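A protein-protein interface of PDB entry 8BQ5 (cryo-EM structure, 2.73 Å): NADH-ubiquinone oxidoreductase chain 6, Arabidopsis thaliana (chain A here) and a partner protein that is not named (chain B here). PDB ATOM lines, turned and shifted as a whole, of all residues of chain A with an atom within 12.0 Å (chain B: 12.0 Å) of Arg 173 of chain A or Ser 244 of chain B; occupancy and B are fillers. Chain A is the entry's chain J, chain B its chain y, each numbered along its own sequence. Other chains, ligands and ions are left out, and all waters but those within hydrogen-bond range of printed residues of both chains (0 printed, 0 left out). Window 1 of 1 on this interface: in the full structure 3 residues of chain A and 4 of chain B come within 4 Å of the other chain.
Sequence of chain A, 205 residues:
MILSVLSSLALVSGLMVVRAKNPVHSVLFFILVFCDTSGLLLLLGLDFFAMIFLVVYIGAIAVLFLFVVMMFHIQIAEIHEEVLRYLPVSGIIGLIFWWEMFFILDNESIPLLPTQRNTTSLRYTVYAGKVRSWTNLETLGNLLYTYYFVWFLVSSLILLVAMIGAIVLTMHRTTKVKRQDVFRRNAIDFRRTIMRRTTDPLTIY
The backbone carbonyl oxygen (O) of Ser 244 of chain B is in hydrogen-bond range of the backbone NH (N) of Arg 173 of chain A. The backbone NH of Arg 173 of chain A sits close to the backbone carbonyl oxygen of Met 245 of chain B.
O of Thr 170 of chain A sits at hydrogen-bond distance from ND1 of His 172 of chain A, 3.5 Å away. The backbone NH (N) of Arg 173 of chain A is in hydrogen-bond range of the side-chain sulfur (SD) of Met 171 of chain A (3.6 Å). The side-chain hydroxyl (OG) of Ser 244 of chain B is in hydrogen-bond range of the backbone carbonyl oxygen (O) of Asp 241 of chain B.
Met 171 of chain A touches Met 245 of chain B. His 172 of chain A touches Ser 244 of chain B. CD of Arg 173 of chain A touches O of Leu 246 of chain B (3.7 Å). O of Arg 173 of chain A touches CA of Gly 247 of chain B, 3.3 Å away.
Of chain B, only Met 245 comes within 4 Å of Met 171 of chain A. Of chain B, only Ser 244, Met 245, Leu 246 and Gly 247 come within 4 Å of Arg 173 of chain A. No residue of chain B comes within 4 Å of Thr 174 of chain A. No residue of chain A comes within 4 Å of Asp 243 of chain B. Gly 247 of chain B touches just one residue of chain A: Arg 173 (3.3 Å). No residue of chain A comes within 4 Å of Ile 248 of chain B.
Printed residues of chain B that touch a printed residue of chain A: Ser 244, Met 245, Leu 246 and Gly 247. Of the 9 printed residues of chain A, 3 touch a printed residue of chain B. Hydrophobic or aromatic side chains of chain A that line the printed part of chain B: Met 171 and His 172. Among the printed residues, 6 pairs touch across the chains. Among the printed residues, no Asp or Glu carboxylate lies within 4 Å of a Lys or Arg side-chain nitrogen of the other chain.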
ATOM      1  N   ALA A 166     -28.155  11.025  -2.981  1.00  0.00           N
ATOM      2  CA  ALA A 166     -27.735   9.687  -3.371  1.00  0.00           C
ATOM      3  C   ALA A 166     -26.478   9.739  -4.225  1.00  0.00           C
ATOM      4  O   ALA A 166     -25.549   8.949  -4.021  1.00  0.00           O
ATOM      5  CB  ALA A 166     -28.861   8.976  -4.119  1.00  0.00           C
ATOM      6  N   ILE A 167     -26.418  10.672  -5.177  1.00  0.00           N
ATOM      7  CA  ILE A 167     -25.225  10.751  -6.018  1.00  0.00           C
ATOM      8  C   ILE A 167     -24.017  11.219  -5.215  1.00  0.00           C
ATOM      9  O   ILE A 167     -22.958  10.583  -5.235  1.00  0.00           O
ATOM     10  CB  ILE A 167     -25.466  11.656  -7.233  1.00  0.00           C
ATOM     11  CG1 ILE A 167     -26.359  10.945  -8.230  1.00  0.00           C
ATOM     12  CG2 ILE A 167     -24.144  12.027  -7.885  1.00  0.00           C
ATOM     13  CD1 ILE A 167     -25.996   9.504  -8.486  1.00  0.00           C
ATOM     14  N   VAL A 168     -24.153  12.333  -4.493  1.00  0.00           N
ATOM     15  CA  VAL A 168     -22.974  12.924  -3.866  1.00  0.00           C
ATOM     16  C   VAL A 168     -22.405  12.001  -2.799  1.00  0.00           C
ATOM     17  O   VAL A 168     -21.199  12.030  -2.528  1.00  0.00           O
ATOM     18  CB  VAL A 168     -23.277  14.321  -3.287  1.00  0.00           C
ATOM     19  CG1 VAL A 168     -23.758  15.256  -4.375  1.00  0.00           C
ATOM     20  CG2 VAL A 168     -24.281  14.237  -2.155  1.00  0.00           C
ATOM     21  N   LEU A 169     -23.238  11.160  -2.187  1.00  0.00           N
ATOM     22  CA  LEU A 169     -22.727  10.340  -1.099  1.00  0.00           C
ATOM     23  C   LEU A 169     -22.118   9.023  -1.578  1.00  0.00           C
ATOM     24  O   LEU A 169     -21.145   8.555  -0.981  1.00  0.00           O
ATOM     25  CB  LEU A 169     -23.836  10.085  -0.079  1.00  0.00           C
ATOM     26  CG  LEU A 169     -24.291  11.364   0.637  1.00  0.00           C
ATOM     27  CD1 LEU A 169     -25.710  11.255   1.172  1.00  0.00           C
ATOM     28  CD2 LEU A 169     -23.328  11.736   1.750  1.00  0.00           C
ATOM     29  N   THR A 170     -22.637   8.419  -2.649  1.00  0.00           N
ATOM     30  CA  THR A 170     -22.222   7.069  -3.010  1.00  0.00           C
ATOM     31  C   THR A 170     -21.476   6.942  -4.332  1.00  0.00           C
ATOM     32  O   THR A 170     -20.870   5.892  -4.565  1.00  0.00           O
ATOM     33  CB  THR A 170     -23.436   6.126  -3.059  1.00  0.00           C
ATOM     34  OG1 THR A 170     -24.344   6.560  -4.078  1.00  0.00           O
ATOM     35  CG2 THR A 170     -24.150   6.106  -1.719  1.00  0.00           C
ATOM     36  N   MET A 171     -21.494   7.955  -5.192  1.00  0.00           N
ATOM     37  CA  MET A 171     -20.978   7.797  -6.548  1.00  0.00           C
ATOM     38  C   MET A 171     -19.458   7.676  -6.561  1.00  0.00           C
ATOM     39  O   MET A 171     -18.749   8.524  -6.015  1.00  0.00           O
ATOM     40  CB  MET A 171     -21.414   8.979  -7.413  1.00  0.00           C
ATOM     41  CG  MET A 171     -20.925   8.942  -8.853  1.00  0.00           C
ATOM     42  SD  MET A 171     -20.874   7.293  -9.577  1.00  0.00           S
ATOM     43  CE  MET A 171     -22.449   7.262 -10.420  1.00  0.00           C
ATOM     44  N   HIS A 172     -18.963   6.617  -7.205  1.00  0.00           N
ATOM     45  CA  HIS A 172     -17.546   6.449  -7.525  1.00  0.00           C
ATOM     46  C   HIS A 172     -17.466   6.137  -9.015  1.00  0.00           C
ATOM     47  O   HIS A 172     -17.553   4.972  -9.409  1.00  0.00           O
ATOM     48  CB  HIS A 172     -16.903   5.333  -6.710  1.00  0.00           C
ATOM     49  CG  HIS A 172     -16.524   5.731  -5.319  1.00  0.00           C
ATOM     50  ND1 HIS A 172     -17.424   5.735  -4.276  1.00  0.00           N
ATOM     51  CD2 HIS A 172     -15.339   6.122  -4.797  1.00  0.00           C
ATOM     52  CE1 HIS A 172     -16.810   6.121  -3.172  1.00  0.00           C
ATOM     53  NE2 HIS A 172     -15.544   6.361  -3.461  1.00  0.00           N
ATOM     54  N   ARG A 173     -17.302   7.165  -9.841  1.00  0.00           N
ATOM     55  CA  ARG A 173     -17.306   6.960 -11.283  1.00  0.00           C
ATOM     56  C   ARG A 173     -16.064   6.195 -11.722  1.00  0.00           C
ATOM     57  O   ARG A 173     -14.983   6.354 -11.148  1.00  0.00           O
ATOM     58  CB  ARG A 173     -17.392   8.296 -12.015  1.00  0.00           C
ATOM     59  CG  ARG A 173     -17.826   8.170 -13.467  1.00  0.00           C
ATOM     60  CD  ARG A 173     -18.061   9.533 -14.088  1.00  0.00           C
ATOM     61  NE  ARG A 173     -18.730   9.437 -15.379  1.00  0.00           N
ATOM     62  CZ  ARG A 173     -19.408  10.426 -15.945  1.00  0.00           C
ATOM     63  NH1 ARG A 173     -19.533  11.603 -15.356  1.00  0.00           N
ATOM     64  NH2 ARG A 173     -19.978  10.227 -17.129  1.00  0.00           N
ATOM     65  N   THR A 174     -16.224   5.366 -12.748  1.00  0.00           N
ATOM     66  CA  THR A 174     -15.138   4.548 -13.271  1.00  0.00           C
ATOM     67  C   THR A 174     -14.362   5.270 -14.367  1.00  0.00           C
ATOM     68  O   THR A 174     -13.135   5.203 -14.417  1.00  0.00           O
ATOM     69  CB  THR A 174     -15.665   3.217 -13.826  1.00  0.00           C
ATOM     70  OG1 THR A 174     -16.416   3.462 -15.020  1.00  0.00           O
ATOM     71  CG2 THR A 174     -16.551   2.527 -12.804  1.00  0.00           C
ATOM     72  N   LYS B 238      -5.430  18.903  -2.112  1.00  0.00           N
ATOM     73  CA  LYS B 238      -6.099  17.877  -2.902  1.00  0.00           C
ATOM     74  C   LYS B 238      -7.468  17.569  -2.309  1.00  0.00           C
ATOM     75  O   LYS B 238      -7.743  17.857  -1.143  1.00  0.00           O
ATOM     76  CB  LYS B 238      -5.255  16.600  -2.991  1.00  0.00           C
ATOM     77  CG  LYS B 238      -4.365  16.364  -1.786  1.00  0.00           C
ATOM     78  CD  LYS B 238      -3.463  15.161  -2.002  1.00  0.00           C
ATOM     79  CE  LYS B 238      -2.541  15.365  -3.189  1.00  0.00           C
ATOM     80  NZ  LYS B 238      -1.527  14.281  -3.284  1.00  0.00           N
ATOM     81  N   ASP B 239      -8.339  17.005  -3.158  1.00  0.00           N
ATOM     82  CA  ASP B 239      -9.669  16.511  -2.774  1.00  0.00           C
ATOM     83  C   ASP B 239      -9.900  15.169  -3.470  1.00  0.00           C
ATOM     84  O   ASP B 239     -10.881  15.005  -4.197  1.00  0.00           O
ATOM     85  CB  ASP B 239     -10.755  17.509  -3.108  1.00  0.00           C
ATOM     86  CG  ASP B 239     -12.105  17.122  -2.520  1.00  0.00           C
ATOM     87  OD1 ASP B 239     -12.178  16.106  -1.799  1.00  0.00           O
ATOM     88  OD2 ASP B 239     -13.090  17.845  -2.769  1.00  0.00           O
ATOM     89  N   GLU B 240      -8.959  14.237  -3.292  1.00  0.00           N
ATOM     90  CA  GLU B 240      -9.017  12.942  -3.969  1.00  0.00           C
ATOM     91  C   GLU B 240     -10.389  12.272  -3.867  1.00  0.00           C
ATOM     92  O   GLU B 240     -10.744  11.471  -4.736  1.00  0.00           O
ATOM     93  CB  GLU B 240      -7.937  12.022  -3.403  1.00  0.00           C
ATOM     94  CG  GLU B 240      -6.592  12.706  -3.217  1.00  0.00           C
ATOM     95  CD  GLU B 240      -5.931  12.356  -1.897  1.00  0.00           C
ATOM     96  OE1 GLU B 240      -4.825  11.780  -1.923  1.00  0.00           O
ATOM     97  OE2 GLU B 240      -6.517  12.664  -0.836  1.00  0.00           O
ATOM     98  N   ASP B 241     -11.168  12.578  -2.825  1.00  0.00           N
ATOM     99  CA  ASP B 241     -12.507  12.007  -2.702  1.00  0.00           C
ATOM    100  C   ASP B 241     -13.435  12.497  -3.811  1.00  0.00           C
ATOM    101  O   ASP B 241     -14.145  11.700  -4.443  1.00  0.00           O
ATOM    102  CB  ASP B 241     -13.084  12.353  -1.331  1.00  0.00           C
ATOM    103  CG  ASP B 241     -14.228  11.455  -0.940  1.00  0.00           C
ATOM    104  OD1 ASP B 241     -15.064  11.887  -0.122  1.00  0.00           O
ATOM    105  OD2 ASP B 241     -14.289  10.316  -1.448  1.00  0.00           O
ATOM    106  N   TYR B 242     -13.445  13.805  -4.064  1.00  0.00           N
ATOM    107  CA  TYR B 242     -14.257  14.330  -5.154  1.00  0.00           C
ATOM    108  C   TYR B 242     -13.704  13.916  -6.510  1.00  0.00           C
ATOM    109  O   TYR B 242     -14.467  13.768  -7.469  1.00  0.00           O
ATOM    110  CB  TYR B 242     -14.351  15.847  -5.049  1.00  0.00           C
ATOM    111  CG  TYR B 242     -15.548  16.422  -5.759  1.00  0.00           C
ATOM    112  CD1 TYR B 242     -16.813  16.335  -5.198  1.00  0.00           C
ATOM    113  CD2 TYR B 242     -15.414  17.058  -6.982  1.00  0.00           C
ATOM    114  CE1 TYR B 242     -17.910  16.857  -5.840  1.00  0.00           C
ATOM    115  CE2 TYR B 242     -16.505  17.587  -7.631  1.00  0.00           C
ATOM    116  CZ  TYR B 242     -17.753  17.486  -7.054  1.00  0.00           C
ATOM    117  OH  TYR B 242     -18.848  18.009  -7.695  1.00  0.00           O
ATOM    118  N   ASP B 243     -12.386  13.733  -6.612  1.00  0.00           N
ATOM    119  CA  ASP B 243     -11.816  13.194  -7.841  1.00  0.00           C
ATOM    120  C   ASP B 243     -12.333  11.788  -8.105  1.00  0.00           C
ATOM    121  O   ASP B 243     -12.693  11.451  -9.238  1.00  0.00           O
ATOM    122  CB  ASP B 243     -10.291  13.198  -7.761  1.00  0.00           C
ATOM    123  CG  ASP B 243      -9.706  14.589  -7.864  1.00  0.00           C
ATOM    124  OD1 ASP B 243      -9.907  15.238  -8.908  1.00  0.00           O
ATOM    125  OD2 ASP B 243      -9.033  15.031  -6.909  1.00  0.00           O
ATOM    126  N   SER B 244     -12.385  10.954  -7.065  1.00  0.00           N
ATOM    127  CA  SER B 244     -12.902   9.601  -7.225  1.00  0.00           C
ATOM    128  C   SER B 244     -14.384   9.618  -7.573  1.00  0.00           C
ATOM    129  O   SER B 244     -14.858   8.768  -8.335  1.00  0.00           O
ATOM    130  CB  SER B 244     -12.650   8.786  -5.958  1.00  0.00           C
ATOM    131  OG  SER B 244     -13.721   8.917  -5.045  1.00  0.00           O
ATOM    132  N   MET B 245     -15.136  10.573  -7.019  1.00  0.00           N
ATOM    133  CA  MET B 245     -16.526  10.719  -7.441  1.00  0.00           C
ATOM    134  C   MET B 245     -16.612  11.100  -8.914  1.00  0.00           C
ATOM    135  O   MET B 245     -17.491  10.620  -9.639  1.00  0.00           O
ATOM    136  CB  MET B 245     -17.254  11.755  -6.585  1.00  0.00           C
ATOM    137  CG  MET B 245     -18.751  11.817  -6.882  1.00  0.00           C
ATOM    138  SD  MET B 245     -19.536  13.392  -6.507  1.00  0.00           S
ATOM    139  CE  MET B 245     -19.069  14.336  -7.951  1.00  0.00           C
ATOM    140  N   LEU B 246     -15.707  11.966  -9.375  1.00  0.00           N
ATOM    141  CA  LEU B 246     -15.673  12.371 -10.775  1.00  0.00           C
ATOM    142  C   LEU B 246     -15.021  11.334 -11.678  1.00  0.00           C
ATOM    143  O   LEU B 246     -15.118  11.459 -12.902  1.00  0.00           O
ATOM    144  CB  LEU B 246     -14.927  13.696 -10.924  1.00  0.00           C
ATOM    145  CG  LEU B 246     -15.681  14.989 -10.621  1.00  0.00           C
ATOM    146  CD1 LEU B 246     -14.689  16.088 -10.319  1.00  0.00           C
ATOM    147  CD2 LEU B 246     -16.567  15.381 -11.785  1.00  0.00           C
ATOM    148  N   GLY B 247     -14.351  10.335 -11.113  1.00  0.00           N
ATOM    149  CA  GLY B 247     -13.670   9.333 -11.915  1.00  0.00           C
ATOM    150  C   GLY B 247     -12.415   9.823 -12.608  1.00  0.00           C
ATOM    151  O   GLY B 247     -12.123   9.391 -13.730  1.00  0.00           O
ATOM    152  N   ILE B 248     -11.661  10.714 -11.966  1.00  0.00           N
ATOM    153  CA  ILE B 248     -10.439  11.263 -12.537  1.00  0.00           C
ATOM    154  C   ILE B 248      -9.316  11.138 -11.517  1.00  0.00           C
ATOM    155  O   ILE B 248      -9.545  11.001 -10.314  1.00  0.00           O
ATOM    156  CB  ILE B 248     -10.601  12.735 -12.971  1.00  0.00           C
ATOM    157  CG1 ILE B 248     -10.818  13.627 -11.748  1.00  0.00           C
ATOM    158  CG2 ILE B 248     -11.743  12.886 -13.955  1.00  0.00           C
ATOM    159  CD1 ILE B 248     -10.547  15.086 -12.008  1.00  0.00           C
ATOM    160  N   THR B 249      -8.085  11.187 -12.020  1.00  0.00           N
ATOM    161  CA  THR B 249      -6.892  11.135 -11.182  1.00  0.00           C
ATOM    162  C   THR B 249      -6.001  12.312 -11.555  1.00  0.00           C
ATOM    163  O   THR B 249      -5.535  12.405 -12.694  1.00  0.00           O
ATOM    164  CB  THR B 249      -6.144   9.813 -11.351  1.00  0.00           C
ATOM    165  OG1 THR B 249      -7.080   8.757 -11.597  1.00  0.00           O
ATOM    166  CG2 THR B 249      -5.350   9.495 -10.095  1.00  0.00           C
ATOM    167  N   ARG B 250      -5.764  13.203 -10.597  1.00  0.00           N
ATOM    168  CA  ARG B 250      -4.948  14.381 -10.842  1.00  0.00           C
ATOM    169  C   ARG B 250      -3.483  14.070 -10.574  1.00  0.00           C
ATOM    170  O   ARG B 250      -3.123  13.608  -9.487  1.00  0.00           O
ATOM    171  CB  ARG B 250      -5.417  15.543  -9.971  1.00  0.00           C
ATOM    172  CG  ARG B 250      -6.893  15.847 -10.134  1.00  0.00           C
ATOM    173  CD  ARG B 250      -7.220  17.259  -9.708  1.00  0.00           C
ATOM    174  NE  ARG B 250      -8.657  17.504  -9.709  1.00  0.00           N
ATOM    175  CZ  ARG B 250      -9.306  18.123 -10.685  1.00  0.00           C
ATOM    176  NH1 ARG B 250      -8.675  18.581 -11.754  1.00  0.00           N
ATOM    177  NH2 ARG B 250     -10.622  18.285 -10.587  1.00  0.00           N
ATOM    178  N   GLU B 251      -2.641  14.329 -11.568  1.00  0.00           N
ATOM    179  CA  GLU B 251      -1.227  13.998 -11.516  1.00  0.00           C
ATOM    180  C   GLU B 251      -0.396  15.266 -11.381  1.00  0.00           C
ATOM    181  O   GLU B 251      -0.707  16.293 -11.992  1.00  0.00           O
ATOM    182  CB  GLU B 251      -0.802  13.228 -12.770  1.00  0.00           C
ATOM    183  CG  GLU B 251      -1.186  11.756 -12.766  1.00  0.00           C
ATOM    184  CD  GLU B 251      -0.418  10.948 -11.735  1.00  0.00           C
ATOM    185  OE1 GLU B 251      -0.871   9.835 -11.393  1.00  0.00           O
ATOM    186  OE2 GLU B 251       0.639  11.423 -11.268  1.00  0.00           O
